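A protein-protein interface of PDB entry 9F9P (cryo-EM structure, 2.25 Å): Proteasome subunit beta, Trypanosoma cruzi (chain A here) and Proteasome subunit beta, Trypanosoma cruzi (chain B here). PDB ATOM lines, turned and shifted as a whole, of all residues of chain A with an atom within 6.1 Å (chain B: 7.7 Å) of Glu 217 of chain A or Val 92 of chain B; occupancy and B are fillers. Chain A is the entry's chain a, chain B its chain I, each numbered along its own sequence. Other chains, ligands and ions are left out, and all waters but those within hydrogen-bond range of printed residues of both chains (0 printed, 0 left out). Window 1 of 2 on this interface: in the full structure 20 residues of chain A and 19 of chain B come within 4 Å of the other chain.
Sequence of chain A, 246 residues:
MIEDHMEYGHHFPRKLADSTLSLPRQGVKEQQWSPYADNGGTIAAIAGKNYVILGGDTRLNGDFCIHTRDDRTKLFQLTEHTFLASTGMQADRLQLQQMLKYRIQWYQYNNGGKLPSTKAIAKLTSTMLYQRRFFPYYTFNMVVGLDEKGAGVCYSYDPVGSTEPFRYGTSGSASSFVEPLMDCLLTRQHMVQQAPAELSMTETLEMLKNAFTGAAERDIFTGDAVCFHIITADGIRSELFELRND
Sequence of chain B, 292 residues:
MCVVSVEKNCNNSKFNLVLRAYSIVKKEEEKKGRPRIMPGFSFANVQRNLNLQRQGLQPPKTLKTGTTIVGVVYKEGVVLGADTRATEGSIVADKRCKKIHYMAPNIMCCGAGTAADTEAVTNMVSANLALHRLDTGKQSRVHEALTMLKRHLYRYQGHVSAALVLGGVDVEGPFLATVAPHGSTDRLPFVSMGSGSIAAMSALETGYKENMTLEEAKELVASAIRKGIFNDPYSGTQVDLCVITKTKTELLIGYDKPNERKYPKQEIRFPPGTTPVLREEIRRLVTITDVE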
ATOM      1  N   PHE A 212      38.220   4.245  17.673  1.00  0.00           N
ATOM      2  CA  PHE A 212      37.538   4.030  18.925  1.00  0.00           C
ATOM      3  C   PHE A 212      36.465   5.090  19.124  1.00  0.00           C
ATOM      4  O   PHE A 212      35.433   4.807  19.694  1.00  0.00           O
ATOM      5  CB  PHE A 212      38.544   4.017  20.075  1.00  0.00           C
ATOM      6  CG  PHE A 212      39.110   2.661  20.385  1.00  0.00           C
ATOM      7  CD1 PHE A 212      38.368   1.746  21.120  1.00  0.00           C
ATOM      8  CD2 PHE A 212      40.371   2.293  19.949  1.00  0.00           C
ATOM      9  CE1 PHE A 212      38.877   0.480  21.417  1.00  0.00           C
ATOM     10  CE2 PHE A 212      40.884   1.035  20.254  1.00  0.00           C
ATOM     11  CZ  PHE A 212      40.148   0.130  21.004  1.00  0.00           C
ATOM     12  N   THR A 213      36.728   6.331  18.715  1.00  0.00           N
ATOM     13  CA  THR A 213      35.737   7.393  18.831  1.00  0.00           C
ATOM     14  C   THR A 213      34.474   7.040  18.027  1.00  0.00           C
ATOM     15  O   THR A 213      33.374   7.059  18.561  1.00  0.00           O
ATOM     16  CB  THR A 213      36.360   8.730  18.426  1.00  0.00           C
ATOM     17  OG1 THR A 213      37.383   9.120  19.346  1.00  0.00           O
ATOM     18  CG2 THR A 213      35.324   9.821  18.414  1.00  0.00           C
ATOM     19  N   GLY A 214      34.644   6.599  16.766  1.00  0.00           N
ATOM     20  CA  GLY A 214      33.540   6.073  15.976  1.00  0.00           C
ATOM     21  C   GLY A 214      32.790   4.885  16.593  1.00  0.00           C
ATOM     22  O   GLY A 214      31.565   4.847  16.573  1.00  0.00           O
ATOM     23  N   ALA A 215      33.510   3.892  17.112  1.00  0.00           N
ATOM     24  CA  ALA A 215      32.903   2.763  17.806  1.00  0.00           C
ATOM     25  C   ALA A 215      32.111   3.173  19.045  1.00  0.00           C
ATOM     26  O   ALA A 215      31.135   2.509  19.380  1.00  0.00           O
ATOM     27  CB  ALA A 215      33.959   1.751  18.240  1.00  0.00           C
ATOM     28  N   ALA A 216      32.585   4.163  19.786  1.00  0.00           N
ATOM     29  CA  ALA A 216      31.879   4.587  20.980  1.00  0.00           C
ATOM     30  C   ALA A 216      30.542   5.257  20.635  1.00  0.00           C
ATOM     31  O   ALA A 216      29.575   5.033  21.348  1.00  0.00           O
ATOM     32  CB  ALA A 216      32.770   5.466  21.838  1.00  0.00           C
ATOM     33  N   GLU A 217      30.451   5.991  19.514  1.00  0.00           N
ATOM     34  CA  GLU A 217      29.197   6.571  19.032  1.00  0.00           C
ATOM     35  C   GLU A 217      28.152   5.541  18.574  1.00  0.00           C
ATOM     36  O   GLU A 217      26.966   5.842  18.624  1.00  0.00           O
ATOM     37  CB  GLU A 217      29.412   7.437  17.795  1.00  0.00           C
ATOM     38  CG  GLU A 217      30.337   8.630  17.998  1.00  0.00           C
ATOM     39  CD  GLU A 217      29.684   9.971  18.288  1.00  0.00           C
ATOM     40  OE1 GLU A 217      30.410  10.889  18.751  1.00  0.00           O
ATOM     41  OE2 GLU A 217      28.465  10.110  18.023  1.00  0.00           O
ATOM     42  N   ARG A 218      28.528   4.351  18.117  1.00  0.00           N
ATOM     43  CA  ARG A 218      27.565   3.474  17.466  1.00  0.00           C
ATOM     44  C   ARG A 218      27.357   2.119  18.149  1.00  0.00           C
ATOM     45  O   ARG A 218      26.388   1.437  17.867  1.00  0.00           O
ATOM     46  CB  ARG A 218      27.990   3.251  16.015  1.00  0.00           C
ATOM     47  CG  ARG A 218      27.901   4.509  15.148  1.00  0.00           C
ATOM     48  CD  ARG A 218      26.496   4.898  14.695  1.00  0.00           C
ATOM     49  NE  ARG A 218      26.395   6.175  13.999  1.00  0.00           N
ATOM     50  CZ  ARG A 218      25.276   6.660  13.436  1.00  0.00           C
ATOM     51  NH1 ARG A 218      24.087   6.125  13.696  1.00  0.00           N
ATOM     52  NH2 ARG A 218      25.353   7.718  12.638  1.00  0.00           N
ATOM     53  N   ASP A 219      28.244   1.694  19.042  1.00  0.00           N
ATOM     54  CA  ASP A 219      28.025   0.482  19.824  1.00  0.00           C
ATOM     55  C   ASP A 219      27.607   0.874  21.228  1.00  0.00           C
ATOM     56  O   ASP A 219      28.247   1.715  21.846  1.00  0.00           O
ATOM     57  CB  ASP A 219      29.291  -0.370  19.888  1.00  0.00           C
ATOM     58  CG  ASP A 219      29.143  -1.673  20.668  1.00  0.00           C
ATOM     59  OD1 ASP A 219      28.091  -2.375  20.501  1.00  0.00           O
ATOM     60  OD2 ASP A 219      30.112  -2.018  21.408  1.00  0.00           O
ATOM     61  N   ILE A 220      26.543   0.275  21.737  1.00  0.00           N
ATOM     62  CA  ILE A 220      26.066   0.691  23.052  1.00  0.00           C
ATOM     63  C   ILE A 220      26.929   0.142  24.190  1.00  0.00           C
ATOM     64  O   ILE A 220      26.865   0.712  25.260  1.00  0.00           O
ATOM     65  CB  ILE A 220      24.592   0.324  23.266  1.00  0.00           C
ATOM     66  CG1 ILE A 220      24.399  -1.181  23.303  1.00  0.00           C
ATOM     67  CG2 ILE A 220      23.716   0.992  22.215  1.00  0.00           C
ATOM     68  CD1 ILE A 220      22.939  -1.595  23.566  1.00  0.00           C
ATOM     69  N   THR A 222      30.400  -0.006  24.326  1.00  0.00           N
ATOM     70  CA  THR A 222      31.788   0.420  24.266  1.00  0.00           C
ATOM     71  C   THR A 222      31.808   1.895  24.587  1.00  0.00           C
ATOM     72  O   THR A 222      31.033   2.629  23.985  1.00  0.00           O
ATOM     73  CB  THR A 222      32.351   0.136  22.864  1.00  0.00           C
ATOM     74  OG1 THR A 222      32.481  -1.276  22.690  1.00  0.00           O
ATOM     75  CG2 THR A 222      33.689   0.806  22.611  1.00  0.00           C
ATOM     76  N   ARG A 244      32.969   9.234  24.834  1.00  0.00           N
ATOM     77  CA  ARG A 244      31.599   9.461  25.271  1.00  0.00           C
ATOM     78  C   ARG A 244      31.148   8.489  26.367  1.00  0.00           C
ATOM     79  O   ARG A 244      31.325   7.277  26.265  1.00  0.00           O
ATOM     80  CB  ARG A 244      30.653   9.298  24.073  1.00  0.00           C
ATOM     81  CG  ARG A 244      30.414  10.595  23.313  1.00  0.00           C
ATOM     82  CD  ARG A 244      29.464  10.435  22.134  1.00  0.00           C
ATOM     83  NE  ARG A 244      28.103  10.129  22.540  1.00  0.00           N
ATOM     84  CZ  ARG A 244      27.023  10.459  21.844  1.00  0.00           C
ATOM     85  NH1 ARG A 244      25.818  10.276  22.353  1.00  0.00           N
ATOM     86  NH2 ARG A 244      27.148  11.015  20.654  1.00  0.00           N
ATOM     87  N   THR B  84      16.805  10.482  22.926  1.00  0.00           N
ATOM     88  CA  THR B  84      16.638  10.435  21.477  1.00  0.00           C
ATOM     89  C   THR B  84      17.354   9.302  20.752  1.00  0.00           C
ATOM     90  O   THR B  84      17.501   9.367  19.560  1.00  0.00           O
ATOM     91  CB  THR B  84      17.162  11.717  20.819  1.00  0.00           C
ATOM     92  OG1 THR B  84      18.587  11.754  20.904  1.00  0.00           O
ATOM     93  CG2 THR B  84      16.638  12.976  21.475  1.00  0.00           C
ATOM     94  N   ARG B  85      17.791   8.265  21.423  1.00  0.00           N
ATOM     95  CA  ARG B  85      18.514   7.193  20.775  1.00  0.00           C
ATOM     96  C   ARG B  85      17.531   6.137  20.301  1.00  0.00           C
ATOM     97  O   ARG B  85      16.674   5.729  21.063  1.00  0.00           O
ATOM     98  CB  ARG B  85      19.474   6.600  21.826  1.00  0.00           C
ATOM     99  CG  ARG B  85      20.123   5.278  21.434  1.00  0.00           C
ATOM    100  CD  ARG B  85      21.141   4.725  22.429  1.00  0.00           C
ATOM    101  NE  ARG B  85      22.326   5.555  22.511  1.00  0.00           N
ATOM    102  CZ  ARG B  85      23.310   5.302  23.362  1.00  0.00           C
ATOM    103  NH1 ARG B  85      23.268   4.202  24.093  1.00  0.00           N
ATOM    104  NH2 ARG B  85      24.315   6.138  23.494  1.00  0.00           N
ATOM    105  N   ALA B  86      17.699   5.628  19.090  1.00  0.00           N
ATOM    106  CA  ALA B  86      17.053   4.384  18.670  1.00  0.00           C
ATOM    107  C   ALA B  86      18.084   3.296  18.402  1.00  0.00           C
ATOM    108  O   ALA B  86      19.065   3.543  17.729  1.00  0.00           O
ATOM    109  CB  ALA B  86      16.274   4.637  17.398  1.00  0.00           C
ATOM    110  N   THR B  87      17.813   2.078  18.835  1.00  0.00           N
ATOM    111  CA  THR B  87      18.721   0.959  18.647  1.00  0.00           C
ATOM    112  C   THR B  87      18.055  -0.166  17.867  1.00  0.00           C
ATOM    113  O   THR B  87      16.854  -0.379  18.003  1.00  0.00           O
ATOM    114  CB  THR B  87      19.196   0.352  19.989  1.00  0.00           C
ATOM    115  OG1 THR B  87      18.095  -0.225  20.692  1.00  0.00           O
ATOM    116  CG2 THR B  87      19.896   1.332  20.911  1.00  0.00           C
ATOM    117  N   GLU B  88      18.876  -0.928  17.119  1.00  0.00           N
ATOM    118  CA  GLU B  88      18.550  -2.289  16.702  1.00  0.00           C
ATOM    119  C   GLU B  88      19.657  -3.216  17.204  1.00  0.00           C
ATOM    120  O   GLU B  88      20.815  -3.093  16.840  1.00  0.00           O
ATOM    121  CB  GLU B  88      18.255  -2.372  15.194  1.00  0.00           C
ATOM    122  CG  GLU B  88      19.391  -1.978  14.251  1.00  0.00           C
ATOM    123  CD  GLU B  88      18.982  -1.613  12.819  1.00  0.00           C
ATOM    124  OE1 GLU B  88      17.791  -1.265  12.620  1.00  0.00           O
ATOM    125  OE2 GLU B  88      19.853  -1.672  11.884  1.00  0.00           O
ATOM    126  N   GLY B  89      19.286  -4.157  18.072  1.00  0.00           N
ATOM    127  CA  GLY B  89      20.251  -5.003  18.756  1.00  0.00           C
ATOM    128  C   GLY B  89      21.144  -4.177  19.679  1.00  0.00           C
ATOM    129  O   GLY B  89      20.651  -3.487  20.569  1.00  0.00           O
ATOM    130  N   SER B  90      22.456  -4.229  19.398  1.00  0.00           N
ATOM    131  CA  SER B  90      23.465  -3.518  20.164  1.00  0.00           C
ATOM    132  C   SER B  90      24.020  -2.314  19.400  1.00  0.00           C
ATOM    133  O   SER B  90      24.995  -1.723  19.839  1.00  0.00           O
ATOM    134  CB  SER B  90      24.571  -4.476  20.542  1.00  0.00           C
ATOM    135  OG  SER B  90      25.219  -4.964  19.380  1.00  0.00           O
ATOM    136  N   ILE B  91      23.383  -1.942  18.286  1.00  0.00           N
ATOM    137  CA  ILE B  91      23.820  -0.845  17.434  1.00  0.00           C
ATOM    138  C   ILE B  91      22.888   0.355  17.585  1.00  0.00           C
ATOM    139  O   ILE B  91      21.684   0.188  17.723  1.00  0.00           O
ATOM    140  CB  ILE B  91      23.805  -1.322  15.980  1.00  0.00           C
ATOM    141  CG1 ILE B  91      24.727  -2.522  15.784  1.00  0.00           C
ATOM    142  CG2 ILE B  91      24.140  -0.203  15.010  1.00  0.00           C
ATOM    143  CD1 ILE B  91      24.301  -3.361  14.608  1.00  0.00           C
ATOM    144  N   VAL B  92      23.464   1.552  17.515  1.00  0.00           N
ATOM    145  CA  VAL B  92      22.725   2.792  17.493  1.00  0.00           C
ATOM    146  C   VAL B  92      22.372   3.157  16.051  1.00  0.00           C
ATOM    147  O   VAL B  92      23.131   3.818  15.366  1.00  0.00           O
ATOM    148  CB  VAL B  92      23.533   3.937  18.159  1.00  0.00           C
ATOM    149  CG1 VAL B  92      22.777   5.244  18.082  1.00  0.00           C
ATOM    150  CG2 VAL B  92      23.913   3.667  19.615  1.00  0.00           C
ATOM    151  N   ALA B  93      21.140   2.863  15.660  1.00  0.00           N
ATOM    152  CA  ALA B  93      20.574   3.219  14.358  1.00  0.00           C
ATOM    153  C   ALA B  93      20.404   4.711  14.138  1.00  0.00           C
ATOM    154  O   ALA B  93      20.799   5.228  13.095  1.00  0.00           O
ATOM    155  CB  ALA B  93      19.251   2.533  14.223  1.00  0.00           C
ATOM    156  N   ASP B  94      19.824   5.420  15.106  1.00  0.00           N
ATOM    157  CA  ASP B  94      19.580   6.849  14.926  1.00  0.00           C
ATOM    158  C   ASP B  94      19.943   7.574  16.219  1.00  0.00           C
ATOM    159  O   ASP B  94      19.446   7.230  17.270  1.00  0.00           O
ATOM    160  CB  ASP B  94      18.118   7.059  14.493  1.00  0.00           C
ATOM    161  CG  ASP B  94      17.649   8.467  14.126  1.00  0.00           C
ATOM    162  OD1 ASP B  94      18.501   9.380  13.982  1.00  0.00           O
ATOM    163  OD2 ASP B  94      16.389   8.635  13.959  1.00  0.00           O
ATOM    164  N   LYS B  95      20.779   8.582  16.154  1.00  0.00           N
ATOM    165  CA  LYS B  95      21.124   9.267  17.380  1.00  0.00           C
ATOM    166  C   LYS B  95      20.124  10.368  17.725  1.00  0.00           C
ATOM    167  O   LYS B  95      20.179  10.805  18.879  1.00  0.00           O
ATOM    168  CB  LYS B  95      22.491   9.957  17.315  1.00  0.00           C
ATOM    169  CG  LYS B  95      23.661   9.103  16.868  1.00  0.00           C
ATOM    170  CD  LYS B  95      24.935   9.946  16.761  1.00  0.00           C
ATOM    171  CE  LYS B  95      25.931   9.407  15.750  1.00  0.00           C
ATOM    172  NZ  LYS B  95      26.933  10.432  15.366  1.00  0.00           N
ATOM    173  N   ARG B  96      19.283  10.825  16.775  1.00  0.00           N
ATOM    174  CA  ARG B  96      18.260  11.832  17.047  1.00  0.00           C
ATOM    175  C   ARG B  96      16.858  11.458  16.562  1.00  0.00           C
ATOM    176  O   ARG B  96      16.276  12.185  15.780  1.00  0.00           O
ATOM    177  CB  ARG B  96      18.598  13.156  16.370  1.00  0.00           C
ATOM    178  CG  ARG B  96      19.872  13.793  16.891  1.00  0.00           C
ATOM    179  CD  ARG B  96      20.312  15.038  16.128  1.00  0.00           C
ATOM    180  NE  ARG B  96      21.771  15.120  16.176  1.00  0.00           N
ATOM    181  CZ  ARG B  96      22.502  15.125  17.297  1.00  0.00           C
ATOM    182  NH1 ARG B  96      23.802  14.896  17.244  1.00  0.00           N
ATOM    183  NH2 ARG B  96      21.921  15.286  18.476  1.00  0.00           N
ATOM    184  N   PRO B 233      21.910   1.394  29.039  1.00  0.00           N
ATOM    185  CA  PRO B 233      22.537   1.300  27.724  1.00  0.00           C
ATOM    186  C   PRO B 233      21.642   1.548  26.519  1.00  0.00           C
ATOM    187  O   PRO B 233      22.145   1.983  25.483  1.00  0.00           O
ATOM    188  CB  PRO B 233      23.086  -0.120  27.642  1.00  0.00           C
ATOM    189  CG  PRO B 233      22.443  -0.868  28.795  1.00  0.00           C
ATOM    190  CD  PRO B 233      22.052   0.168  29.831  1.00  0.00           C
ATOM    191  N   SER B 235      19.400   3.969  26.291  1.00  0.00           N
ATOM    192  CA  SER B 235      18.984   5.362  26.219  1.00  0.00           C
ATOM    193  C   SER B 235      20.191   6.251  25.996  1.00  0.00           C
ATOM    194  O   SER B 235      21.263   5.917  26.448  1.00  0.00           O
ATOM    195  CB  SER B 235      18.289   5.823  27.488  1.00  0.00           C
ATOM    196  OG  SER B 235      17.217   4.973  27.820  1.00  0.00           O
ATOM    197  N   GLY B 236      20.022   7.416  25.405  1.00  0.00           N
ATOM    198  CA  GLY B 236      21.197   8.203  25.128  1.00  0.00           C
ATOM    199  C   GLY B 236      20.936   9.498  24.363  1.00  0.00           C
ATOM    200  O   GLY B 236      19.816   9.844  24.083  1.00  0.00           O
ATOM    201  N   THR B 237      22.055  10.195  24.149  1.00  0.00           N
ATOM    202  CA  THR B 237      22.293  11.369  23.341  1.00  0.00           C
ATOM    203  C   THR B 237      21.849  12.674  23.985  1.00  0.00           C
ATOM    204  O   THR B 237      22.706  13.415  24.444  1.00  0.00           O
ATOM    205  CB  THR B 237      21.720  11.302  21.936  1.00  0.00           C
ATOM    206  OG1 THR B 237      22.131  10.110  21.274  1.00  0.00           O
ATOM    207  CG2 THR B 237      22.152  12.533  21.157  1.00  0.00           C
ATOM    208  N   ASN B 259      26.667  15.482  25.806  1.00  0.00           N
ATOM    209  CA  ASN B 259      27.518  14.482  25.167  1.00  0.00           C
ATOM    210  C   ASN B 259      28.049  14.987  23.830  1.00  0.00           C
ATOM    211  O   ASN B 259      27.779  14.384  22.791  1.00  0.00           O
ATOM    212  CB  ASN B 259      26.778  13.174  24.860  1.00  0.00           C
ATOM    213  CG  ASN B 259      26.572  12.273  26.058  1.00  0.00           C
ATOM    214  OD1 ASN B 259      27.532  11.861  26.713  1.00  0.00           O
ATOM    215  ND2 ASN B 259      25.320  11.940  26.327  1.00  0.00           N
ATOM    216  N   GLU B 260      28.838  16.067  23.861  1.00  0.00           N
ATOM    217  CA  GLU B 260      29.463  16.599  22.655  1.00  0.00           C
ATOM    218  C   GLU B 260      30.667  15.742  22.252  1.00  0.00           C
ATOM    219  O   GLU B 260      30.943  14.702  22.852  1.00  0.00           O
ATOM    220  CB  GLU B 260      29.835  18.072  22.867  1.00  0.00           C
ATOM    221  CG  GLU B 260      28.887  19.050  22.182  1.00  0.00           C
ATOM    222  CD  GLU B 260      27.416  18.938  22.549  1.00  0.00           C
ATOM    223  OE1 GLU B 260      26.597  19.645  21.927  1.00  0.00           O
ATOM    224  OE2 GLU B 260      27.090  18.149  23.456  1.00  0.00           O
ATOM    225  N   ARG B 261      31.363  16.184  21.195  1.00  0.00           N
ATOM    226  CA  ARG B 261      32.585  15.549  20.721  1.00  0.00           C
ATOM    227  C   ARG B 261      33.769  15.995  21.584  1.00  0.00           C
ATOM    228  O   ARG B 261      33.888  17.172  21.933  1.00  0.00           O
ATOM    229  CB  ARG B 261      32.780  15.861  19.228  1.00  0.00           C
ATOM    230  CG  ARG B 261      32.413  14.718  18.291  1.00  0.00           C
ATOM    231  CD  ARG B 261      33.625  13.831  18.092  1.00  0.00           C
ATOM    232  NE  ARG B 261      33.412  12.554  17.425  1.00  0.00           N
ATOM    233  CZ  ARG B 261      33.127  12.398  16.137  1.00  0.00           C
ATOM    234  NH1 ARG B 261      32.714  13.429  15.423  1.00  0.00           N
ATOM    235  NH2 ARG B 261      33.206  11.198  15.581  1.00  0.00           N
ATOM    236  N   LYS B 262      34.638  15.027  21.923  1.00  0.00           N
ATOM    237  CA  LYS B 262      35.803  15.243  22.772  1.00  0.00           C
ATOM    238  C   LYS B 262      37.049  15.437  21.902  1.00  0.00           C
ATOM    239  O   LYS B 262      37.818  16.376  22.110  1.00  0.00           O
ATOM    240  CB  LYS B 262      35.968  14.060  23.739  1.00  0.00           C
ATOM    241  CG  LYS B 262      34.701  13.678  24.500  1.00  0.00           C
ATOM    242  CD  LYS B 262      34.928  13.057  25.865  1.00  0.00           C
ATOM    243  CE  LYS B 262      33.831  13.411  26.852  1.00  0.00           C
ATOM    244  NZ  LYS B 262      34.105  12.884  28.210  1.00  0.00           N
ATOM    245  N   TYR B 263      37.225  14.522  20.937  1.00  0.00           N
ATOM    246  CA  TYR B 263      38.304  14.540  19.959  1.00  0.00           C
ATOM    247  C   TYR B 263      37.696  14.820  18.582  1.00  0.00           C
ATOM    248  O   TYR B 263      36.876  14.033  18.110  1.00  0.00           O
ATOM    249  CB  TYR B 263      39.035  13.191  20.037  1.00  0.00           C
ATOM    250  CG  TYR B 263      40.323  13.006  19.257  1.00  0.00           C
ATOM    251  CD1 TYR B 263      41.525  13.577  19.670  1.00  0.00           C
ATOM    252  CD2 TYR B 263      40.362  12.166  18.146  1.00  0.00           C
ATOM    253  CE1 TYR B 263      42.710  13.364  18.973  1.00  0.00           C
ATOM    254  CE2 TYR B 263      41.534  11.950  17.437  1.00  0.00           C
ATOM    255  CZ  TYR B 263      42.715  12.550  17.847  1.00  0.00           C
ATOM    256  OH  TYR B 263      43.869  12.307  17.124  1.00  0.00           O
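OE2 of Glu 217 of chain A lies within salt-bridge range of NZ of Lys 95 of chain B (3.1 Å). The backbone NH (N) of Ile 220 of chain A sits at hydrogen-bond distance from the backbone carbonyl oxygen (O) of Ser 90 of chain B (3.2 Å). OD1 of Asp 219 of chain A sits close to O of Ser 90 of chain B, 3.2 Å away. The side-chain carboxylate of Glu 217 of chain A is in salt-bridge range of the guanidinium group of Arg 261 of chain B (3.7 Å). O of Arg 218 of chain A sits at hydrogen-bond distance from N of Val 92 of chain B (2.9 Å). The guanidinium group of Arg 218 of chain A lies within hydrogen-bond range of the backbone carbonyl oxygen of Ala 93 of chain B.
The side-chain hydroxyl (OG1) of Thr 84 of chain B lies within hydrogen-bond range of the backbone carbonyl oxygen (O) of Lys 95 of chain B, at 2.7 Å. The side-chain carboxylate (OD2) of Asp 219 of chain A lies within hydrogen-bond range of the side-chain hydroxyl (OG1) of Thr 222 of chain A (2.8 Å). OE2 of Glu 217 of chain A lies within salt-bridge range of NH2 of Arg 244 of chain A, at 3.1 Å. The backbone carbonyl oxygen (O) of Ala 86 of chain B is in hydrogen-bond range of the backbone NH (N) of Ala 93 of chain B (3.0 Å). The guanidinium group of Arg 85 of chain B sits at hydrogen-bond distance from the backbone carbonyl oxygen of Pro 233 of chain B. O of Lys 95 of chain B is in hydrogen-bond range of OG1 of Thr 237 of chain B.
Hydrophobic or aromatic side chains of chain B that line the printed part of chain A: Ile 91 and Val 92. Along chain B the printed residues that touch a printed residue of chain A span positions 85 to 261. Hydrophobic or aromatic side chains of chain A within 4 Å of the printed part of chain B: Ile 220.
CG2 of Thr 213 of chain A touches NE of Arg 261 of chain B (3.5 Å). Glu 217 of chain A touches Val 92 of chain B. Arg 218 of chain A touches Ser 90 of chain B. Arg 218 of chain A touches Ile 91 of chain B (O to CA, 3.5 Å). Arg 218 of chain A touches Lys 95 of chain B (NH2 to CE, 3.6 Å). Arg 85 of chain B touches Ile 220 of chain A (NH1 to CG2, 3.7 Å). Val 92 of chain B touches Ile 220 of chain A (CG2 to CG2, 3.7 Å). Pro 233 of chain B touches Ile 220 of chain A (O to CB, 3.7 Å). NH1 of Arg 244 of chain A touches CA of Thr 237 of chain B, 3.8 Å away. NH1 of Arg 244 of chain A touches CB of Asn 259 of chain B (3.95 Å).
Ala 216 of chain A touches none of the printed residues of chain B. Printed residues of chain B within 4 Å of Asp 219 of chain A: Ser 90 (3.2 Å). Thr 84 of chain B touches none of the printed residues of chain A. Of the printed residues of chain A, Arg 85 of chain B touches Ile 220 (3.7 Å). Val 92 of chain B touches just these residues of chain A: Glu 217, Arg 218 and Ile 220. Asp 94 of chain B touches none of the printed residues of chain A. The nearest residue of chain A that does not touch Val 92 of chain B is Asp 219 of chain A (4.8 Å).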
